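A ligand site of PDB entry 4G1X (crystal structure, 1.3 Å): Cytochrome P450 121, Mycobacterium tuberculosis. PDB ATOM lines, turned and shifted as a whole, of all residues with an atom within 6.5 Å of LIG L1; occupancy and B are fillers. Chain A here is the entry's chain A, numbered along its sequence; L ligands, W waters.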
ATOM      1  N   MET A  61     -29.904  -8.512   5.971  1.00  0.00           N
ATOM      2  CA  MET A  61     -28.838  -8.329   6.946  1.00  0.00           C
ATOM      3  C   MET A  61     -29.395  -7.644   8.144  1.00  0.00           C
ATOM      4  O   MET A  61     -29.120  -8.075   9.299  1.00  0.00           O
ATOM      5  CB  MET A  61     -27.691  -7.505   6.310  1.00  0.00           C
ATOM      6  CG  MET A  61     -26.624  -7.077   7.310  1.00  0.00           C
ATOM      7  SD  MET A  61     -25.313  -6.040   6.650  1.00  0.00           S
ATOM      8  CE  MET A  61     -24.431  -7.207   5.732  1.00  0.00           C
ATOM      9  N   VAL A  81     -26.249  -0.617  14.460  1.00  0.00           N
ATOM     10  CA  VAL A  81     -25.005  -0.619  13.685  1.00  0.00           C
ATOM     11  C   VAL A  81     -24.918  -1.788  12.757  1.00  0.00           C
ATOM     12  O   VAL A  81     -24.189  -1.822  11.766  1.00  0.00           O
ATOM     13  CB  VAL A  81     -23.803  -0.501  14.652  1.00  0.00           C
ATOM     14  CG1 VAL A  81     -22.465  -0.600  13.872  1.00  0.00           C
ATOM     15  CG2 VAL A  81     -23.836   0.817  15.398  1.00  0.00           C
ATOM     16  N   VAL A  82     -25.798  -2.814  12.929  1.00  0.00           N
ATOM     17  CA  VAL A  82     -25.871  -3.886  11.961  1.00  0.00           C
ATOM     18  C   VAL A  82     -26.387  -3.334  10.605  1.00  0.00           C
ATOM     19  O   VAL A  82     -26.022  -3.912   9.581  1.00  0.00           O
ATOM     20  CB  VAL A  82     -26.756  -5.022  12.549  1.00  0.00           C
ATOM     21  CG1 VAL A  82     -27.019  -6.168  11.495  1.00  0.00           C
ATOM     22  CG2 VAL A  82     -26.014  -5.614  13.765  1.00  0.00           C
ATOM     23  N   ASN A  84     -25.314  -0.562   9.280  1.00  0.00           N
ATOM     24  CA  ASN A  84     -24.420   0.554   9.152  1.00  0.00           C
ATOM     25  C   ASN A  84     -24.459   1.163   7.738  1.00  0.00           C
ATOM     26  O   ASN A  84     -24.631   2.410   7.628  1.00  0.00           O
ATOM     27  CB  ASN A  84     -22.993   0.091   9.508  1.00  0.00           C
ATOM     28  CG  ASN A  84     -22.015   1.223   9.709  1.00  0.00           C
ATOM     29  OD1 ASN A  84     -22.327   2.251  10.352  1.00  0.00           O
ATOM     30  ND2 ASN A  84     -20.790   1.033   9.262  1.00  0.00           N
ATOM     31  N   MET A  85     -24.194   0.392   6.682  1.00  0.00           N
ATOM     32  CA  MET A  85     -24.126   1.017   5.363  1.00  0.00           C
ATOM     33  C   MET A  85     -25.525   1.545   4.999  1.00  0.00           C
ATOM     34  O   MET A  85     -25.575   2.645   4.335  1.00  0.00           O
ATOM     35  CB  MET A  85     -23.566  -0.016   4.345  1.00  0.00           C
ATOM     36  CG  MET A  85     -22.969   0.567   3.013  1.00  0.00           C
ATOM     37  SD  MET A  85     -21.467   1.471   3.382  1.00  0.00           S
ATOM     38  N   ILE A  88     -25.649   4.917   6.643  1.00  0.00           N
ATOM     39  CA  ILE A  88     -24.789   5.843   5.882  1.00  0.00           C
ATOM     40  C   ILE A  88     -25.535   6.301   4.643  1.00  0.00           C
ATOM     41  O   ILE A  88     -25.563   7.588   4.376  1.00  0.00           O
ATOM     42  CB  ILE A  88     -23.466   5.143   5.576  1.00  0.00           C
ATOM     43  CG1 ILE A  88     -22.660   4.951   6.836  1.00  0.00           C
ATOM     44  CG2 ILE A  88     -22.657   5.934   4.485  1.00  0.00           C
ATOM     45  CD1 ILE A  88     -21.456   3.987   6.671  1.00  0.00           C
ATOM     46  N   PHE A 167     -14.060  -8.448  16.953  1.00  0.00           N
ATOM     47  CA  PHE A 167     -14.412  -9.362  15.927  1.00  0.00           C
ATOM     48  C   PHE A 167     -14.499 -10.821  16.365  1.00  0.00           C
ATOM     49  O   PHE A 167     -14.524 -11.744  15.583  1.00  0.00           O
ATOM     50  CB  PHE A 167     -13.547  -9.187  14.658  1.00  0.00           C
ATOM     51  CG  PHE A 167     -13.952  -7.941  13.943  1.00  0.00           C
ATOM     52  CD1 PHE A 167     -13.373  -6.766  14.234  1.00  0.00           C
ATOM     53  CD2 PHE A 167     -14.935  -7.980  12.933  1.00  0.00           C
ATOM     54  CE1 PHE A 167     -13.785  -5.502  13.555  1.00  0.00           C
ATOM     55  CE2 PHE A 167     -15.347  -6.767  12.307  1.00  0.00           C
ATOM     56  CZ  PHE A 167     -14.749  -5.665  12.627  1.00  0.00           C
ATOM     57  N   THR A 228     -16.241   1.745  12.706  1.00  0.00           N
ATOM     58  CA  THR A 228     -16.607   0.554  11.932  1.00  0.00           C
ATOM     59  C   THR A 228     -15.752   0.377  10.709  1.00  0.00           C
ATOM     60  O   THR A 228     -15.374  -0.765  10.346  1.00  0.00           O
ATOM     61  CB  THR A 228     -18.071   0.549  11.516  1.00  0.00           C
ATOM     62  OG1 THR A 228     -18.379   1.749  10.771  1.00  0.00           O
ATOM     63  CG2 THR A 228     -18.997   0.450  12.771  1.00  0.00           C
ATOM     64  N   PHE A 229     -15.438   1.467   9.980  1.00  0.00           N
ATOM     65  CA  PHE A 229     -14.630   1.339   8.793  1.00  0.00           C
ATOM     66  C   PHE A 229     -13.171   1.053   9.185  1.00  0.00           C
ATOM     67  O   PHE A 229     -12.533   0.181   8.499  1.00  0.00           O
ATOM     68  CB  PHE A 229     -14.751   2.587   7.832  1.00  0.00           C
ATOM     69  CG  PHE A 229     -15.958   2.512   6.972  1.00  0.00           C
ATOM     70  CD1 PHE A 229     -17.257   2.387   7.511  1.00  0.00           C
ATOM     71  CD2 PHE A 229     -15.838   2.520   5.613  1.00  0.00           C
ATOM     72  CE1 PHE A 229     -18.351   2.298   6.674  1.00  0.00           C
ATOM     73  CE2 PHE A 229     -16.953   2.436   4.773  1.00  0.00           C
ATOM     74  CZ  PHE A 229     -18.206   2.326   5.324  1.00  0.00           C
ATOM     75  N   ALA A 232     -13.412  -2.891  10.529  1.00  0.00           N
ATOM     76  CA  ALA A 232     -13.729  -3.884   9.507  1.00  0.00           C
ATOM     77  C   ALA A 232     -12.702  -3.906   8.398  1.00  0.00           C
ATOM     78  O   ALA A 232     -12.326  -4.954   7.873  1.00  0.00           O
ATOM     79  CB  ALA A 232     -15.129  -3.684   8.992  1.00  0.00           C
ATOM     80  N   GLY A 233     -12.189  -2.743   8.062  1.00  0.00           N
ATOM     81  CA  GLY A 233     -11.222  -2.681   6.996  1.00  0.00           C
ATOM     82  C   GLY A 233      -9.896  -3.316   7.463  1.00  0.00           C
ATOM     83  O   GLY A 233      -9.278  -4.088   6.704  1.00  0.00           O
ATOM     84  N   ILE A 235      -9.381  -5.501   9.997  1.00  0.00           N
ATOM     85  CA  ILE A 235      -9.473  -6.972  10.221  1.00  0.00           C
ATOM     86  C   ILE A 235      -9.527  -7.659   8.902  1.00  0.00           C
ATOM     87  O   ILE A 235      -9.032  -8.792   8.734  1.00  0.00           O
ATOM     88  CB  ILE A 235     -10.600  -7.291  11.205  1.00  0.00           C
ATOM     89  CG1 ILE A 235     -10.243  -8.598  11.924  1.00  0.00           C
ATOM     90  CG2 ILE A 235     -11.974  -7.418  10.549  1.00  0.00           C
ATOM     91  CD1 ILE A 235      -9.062  -8.564  12.863  1.00  0.00           C
ATOM     92  N   SER A 236     -10.282  -7.125   7.921  1.00  0.00           N
ATOM     93  CA  SER A 236     -10.522  -7.851   6.708  1.00  0.00           C
ATOM     94  C   SER A 236      -9.284  -7.891   5.814  1.00  0.00           C
ATOM     95  O   SER A 236      -8.884  -8.943   5.307  1.00  0.00           O
ATOM     96  CB  SER A 236     -11.669  -7.225   5.893  1.00  0.00           C
ATOM     97  OG  SER A 236     -12.893  -7.275   6.623  1.00  0.00           O
ATOM     98  N   PHE A 279     -12.980 -15.766   6.074  1.00  0.00           N
ATOM     99  CA  PHE A 279     -14.245 -15.692   6.806  1.00  0.00           C
ATOM    100  C   PHE A 279     -14.564 -16.962   7.529  1.00  0.00           C
ATOM    101  O   PHE A 279     -14.642 -17.999   6.941  1.00  0.00           O
ATOM    102  CB  PHE A 279     -15.405 -15.302   5.852  1.00  0.00           C
ATOM    103  CG  PHE A 279     -15.424 -13.841   5.562  1.00  0.00           C
ATOM    104  CD1 PHE A 279     -14.406 -13.244   4.837  1.00  0.00           C
ATOM    105  CD2 PHE A 279     -16.421 -13.023   6.128  1.00  0.00           C
ATOM    106  CE1 PHE A 279     -14.451 -11.841   4.612  1.00  0.00           C
ATOM    107  CE2 PHE A 279     -16.367 -11.613   5.899  1.00  0.00           C
ATOM    108  CZ  PHE A 279     -15.347 -11.090   5.184  1.00  0.00           C
ATOM    109  N   LEU A 283     -21.969 -15.843   5.864  1.00  0.00           N
ATOM    110  CA  LEU A 283     -22.550 -14.525   6.040  1.00  0.00           C
ATOM    111  C   LEU A 283     -24.035 -14.709   6.455  1.00  0.00           C
ATOM    112  O   LEU A 283     -24.774 -15.438   5.792  1.00  0.00           O
ATOM    113  CB  LEU A 283     -22.558 -13.745   4.684  1.00  0.00           C
ATOM    114  CG  LEU A 283     -21.152 -13.591   4.032  1.00  0.00           C
ATOM    115  CD1 LEU A 283     -21.351 -12.794   2.746  1.00  0.00           C
ATOM    116  CD2 LEU A 283     -20.206 -12.908   4.992  1.00  0.00           C
ATOM    117  N   CYS A 344     -18.969  -5.493  -0.806  1.00  0.00           N
ATOM    118  CA  CYS A 344     -17.966  -4.712  -0.026  1.00  0.00           C
ATOM    119  C   CYS A 344     -17.585  -3.349  -0.714  1.00  0.00           C
ATOM    120  O   CYS A 344     -17.041  -3.454  -1.863  1.00  0.00           O
ATOM    121  CB  CYS A 344     -16.694  -5.559   0.093  1.00  0.00           C
ATOM    122  SG  CYS A 344     -15.467  -4.725   1.118  1.00  0.00           S
ATOM    123  N   PRO A 345     -17.773  -2.273  -0.088  1.00  0.00           N
ATOM    124  CA  PRO A 345     -17.330  -0.992  -0.740  1.00  0.00           C
ATOM    125  C   PRO A 345     -15.864  -0.834  -0.620  1.00  0.00           C
ATOM    126  O   PRO A 345     -15.266   0.090  -1.219  1.00  0.00           O
ATOM    127  CB  PRO A 345     -18.105   0.088   0.070  1.00  0.00           C
ATOM    128  CG  PRO A 345     -18.204  -0.566   1.460  1.00  0.00           C
ATOM    129  CD  PRO A 345     -18.504  -2.056   1.176  1.00  0.00           C
ATOM    130  N   GLN A 384     -14.400 -14.006  14.035  1.00  0.00           N
ATOM    131  CA  GLN A 384     -15.090 -13.865  12.735  1.00  0.00           C
ATOM    132  C   GLN A 384     -14.185 -14.066  11.548  1.00  0.00           C
ATOM    133  O   GLN A 384     -14.658 -14.107  10.383  1.00  0.00           O
ATOM    134  CB  GLN A 384     -15.776 -12.499  12.647  1.00  0.00           C
ATOM    135  CG  GLN A 384     -16.919 -12.320  13.684  1.00  0.00           C
ATOM    136  CD  GLN A 384     -17.466 -10.911  13.720  1.00  0.00           C
ATOM    137  OE1 GLN A 384     -17.843 -10.372  14.827  1.00  0.00           O
ATOM    138  NE2 GLN A 384     -17.650 -10.241  12.587  1.00  0.00           N
ATOM    139  N   ARG A 385     -12.881 -14.120  11.771  1.00  0.00           N
ATOM    140  CA  ARG A 385     -11.924 -14.469  10.746  1.00  0.00           C
ATOM    141  C   ARG A 385     -11.130 -15.691  11.111  1.00  0.00           C
ATOM    142  O   ARG A 385     -10.983 -15.954  12.376  1.00  0.00           O
ATOM    143  CB  ARG A 385     -10.941 -13.317  10.428  1.00  0.00           C
ATOM    144  CG  ARG A 385     -11.614 -12.028   9.881  1.00  0.00           C
ATOM    145  CD  ARG A 385     -12.308 -12.295   8.499  1.00  0.00           C
ATOM    146  NE  ARG A 385     -12.897 -11.023   7.951  1.00  0.00           N
ATOM    147  CZ  ARG A 385     -14.013 -10.554   8.367  1.00  0.00           C
ATOM    148  NH1 ARG A 385     -14.432  -9.353   7.907  1.00  0.00           N
ATOM    149  NH2 ARG A 385     -14.826 -11.254   9.218  1.00  0.00           N
HETATM  150  C1  LIG L   1     -18.736  -5.869   7.213  1.00  0.00           C
HETATM  151  C2  LIG L   1     -17.553  -5.345   6.714  1.00  0.00           C
HETATM  152  C3  LIG L   1     -16.652  -6.185   6.065  1.00  0.00           C
HETATM  153  N1  LIG L   1     -15.507  -5.692   5.596  1.00  0.00           N
HETATM  154  C4  LIG L   1     -16.942  -7.537   5.910  1.00  0.00           C
HETATM  155  C5  LIG L   1     -18.132  -8.050   6.402  1.00  0.00           C
HETATM  156  C6  LIG L   1     -19.034  -7.216   7.059  1.00  0.00           C
HETATM  157  N2  LIG L   1     -20.187  -7.721   7.530  1.00  0.00           N
HETATM  158  C7  LIG L   1     -21.066  -6.955   8.156  1.00  0.00           C
HETATM  159  C8  LIG L   1     -20.825  -5.594   8.342  1.00  0.00           C
HETATM  160  C9  LIG L   1     -19.644  -5.041   7.863  1.00  0.00           C
HETATM  161  N3  LIG L   1     -19.390  -3.749   8.028  1.00  0.00           N
HETATM  162  C10 LIG L   1     -20.236  -2.731   7.918  1.00  0.00           C
HETATM  163  N4  LIG L   1     -19.549  -1.619   8.157  1.00  0.00           N
HETATM  164  C11 LIG L   1     -18.304  -2.007   8.413  1.00  0.00           C
HETATM  165  N5  LIG L   1     -18.269  -3.345   8.314  1.00  0.00           N
HETATM  166  C1  LG2 L   2     -18.939  -5.787   3.342  1.00  0.00           C
HETATM  167  C2  LG2 L   2     -15.163  -8.802   2.464  1.00  0.00           C
HETATM  168  C3  LG2 L   2     -12.097  -5.059   2.913  1.00  0.00           C
HETATM  169  C4  LG2 L   2     -15.820  -2.332   4.463  1.00  0.00           C
HETATM  170  C5  LG2 L   2     -18.134  -6.904   2.960  1.00  0.00           C
HETATM  171  C6  LG2 L   2     -18.717  -8.208   2.624  1.00  0.00           C
HETATM  172  C7  LG2 L   2     -17.660  -9.102   2.454  1.00  0.00           C
HETATM  173  C8  LG2 L   2     -16.448  -8.331   2.614  1.00  0.00           C
HETATM  174  C9  LG2 L   2     -17.771 -10.526   2.198  1.00  0.00           C
HETATM  175  C10 LG2 L   2     -20.199  -8.546   2.507  1.00  0.00           C
HETATM  176  C11 LG2 L   2     -20.863  -8.913   3.849  1.00  0.00           C
HETATM  177  C12 LG2 L   2     -22.266  -9.381   3.688  1.00  0.00           C
HETATM  178  O1  LG2 L   2     -22.875  -9.279   2.613  1.00  0.00           O
HETATM  179  O2  LG2 L   2     -22.833  -9.958   4.727  1.00  0.00           O
HETATM  180  C13 LG2 L   2     -14.013  -8.015   2.541  1.00  0.00           C
HETATM  181  C14 LG2 L   2     -12.758  -8.517   2.232  1.00  0.00           C
HETATM  182  C15 LG2 L   2     -11.847  -7.455   2.362  1.00  0.00           C
HETATM  183  C16 LG2 L   2     -12.694  -6.348   2.737  1.00  0.00           C
HETATM  184  C17 LG2 L   2     -12.419  -9.898   1.887  1.00  0.00           C
HETATM  185  C18 LG2 L   2     -10.385  -7.405   2.186  1.00  0.00           C
HETATM  186  C19 LG2 L   2      -9.630  -8.138   1.393  1.00  0.00           C
HETATM  187  C20 LG2 L   2     -12.912  -3.990   3.270  1.00  0.00           C
HETATM  188  C21 LG2 L   2     -12.319  -2.665   3.509  1.00  0.00           C
HETATM  189  C22 LG2 L   2     -13.364  -1.885   4.071  1.00  0.00           C
HETATM  190  C23 LG2 L   2     -14.550  -2.691   4.058  1.00  0.00           C
HETATM  191  C24 LG2 L   2     -10.953  -2.133   3.236  1.00  0.00           C
HETATM  192  C25 LG2 L   2     -13.322  -0.416   4.467  1.00  0.00           C
HETATM  193  C26 LG2 L   2     -12.318   0.436   4.726  1.00  0.00           C
HETATM  194  C27 LG2 L   2     -17.017  -3.039   4.289  1.00  0.00           C
HETATM  195  C28 LG2 L   2     -18.322  -2.476   4.641  1.00  0.00           C
HETATM  196  C29 LG2 L   2     -19.199  -3.471   4.315  1.00  0.00           C
HETATM  197  C30 LG2 L   2     -18.396  -4.580   3.811  1.00  0.00           C
HETATM  198  C31 LG2 L   2     -18.606  -1.118   5.215  1.00  0.00           C
HETATM  199  C32 LG2 L   2     -20.715  -3.479   4.506  1.00  0.00           C
HETATM  200  C33 LG2 L   2     -21.463  -3.137   3.259  1.00  0.00           C
HETATM  201  C34 LG2 L   2     -22.977  -3.237   3.446  1.00  0.00           C
HETATM  202  O3  LG2 L   2     -23.505  -2.786   2.420  1.00  0.00           O
HETATM  203  O4  LG2 L   2     -23.530  -3.705   4.442  1.00  0.00           O
HETATM  204  N1  LG2 L   2     -16.708  -6.978   2.975  1.00  0.00           N
HETATM  205  N2  LG2 L   2     -13.981  -6.727   2.904  1.00  0.00           N
HETATM  206  N3  LG2 L   2     -14.230  -4.024   3.628  1.00  0.00           N
HETATM  207  N4  LG2 L   2     -17.099  -4.272   3.761  1.00  0.00           N
HETATM  208 FE1  LG2 L   2     -15.534  -5.454   3.189  1.00  0.00          FE
HETATM  209  O   HOH W   1     -23.477  -3.761   8.949  1.00  0.00           O
HETATM  210  O   HOH W   2     -23.894  -6.327   9.768  1.00  0.00           O
HETATM  211  O   HOH W   3     -16.680  -8.057   9.300  1.00  0.00           O
HETATM  212  O   HOH W   4     -17.699  -5.514  10.277  1.00  0.00           O
HETATM  213  O   HOH W   5     -21.671 -10.104   7.208  1.00  0.00           O
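Thr 228 touches LIG L1 (O to C11, 3.7 Å).
CB of Ala 232 touches N5 of LIG L1, 3.2 Å away.
Phe 279 touches LIG L1.
Arg 385 touches LIG L1 (NH1 to C4, 3.7 Å).
Hydrophobic or aromatic side chains that line LIG L1: Ala 232 and Phe 279.
Within 4 Å of LIG L1: Asn 84, Thr 228, Ala 232, Ser 236, Phe 279 and Arg 385.
The nearest printed residue that does not touch LIG L1 is Met 61 (4.2 Å).
A nitrogen (N1) of LIG L1 is bound to an iron atom (FE1) of LG2 L2, at 2.4 Å.
The side-chain sulfur of Cys 344 is bound to an iron atom (FE1) of LG2 L2.
The side-chain amide nitrogen (ND2) of Asn 84 sits at hydrogen-bond distance from a nitrogen (N4) of LIG L1 (3.1 Å).
OG of Ser 236 sits close to N1 of LIG L1 (3.2 Å).
Water W5 lies within hydrogen-bond range of an oxygen (O2) of LG2 L2 (2.7 Å) and a nitrogen (N2) of LIG L1 (2.8 Å).
Water W2 bridges the backbone carbonyl oxygen (O) of Val 82 (3.2 Å) and the side-chain sulfur (SD) of Met 61 (3.4 Å).
The side-chain hydroxyl of Thr 228 sits at hydrogen-bond distance from the side-chain amide nitrogen of Asn 84 (2.9 Å).
NH1 of Arg 385 is in hydrogen-bond range of OG of Ser 236 (2.9 Å).
The side-chain hydroxyl of Ser 236 is in hydrogen-bond range of the backbone carbonyl oxygen of Ala 232, at 2.7 Å.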
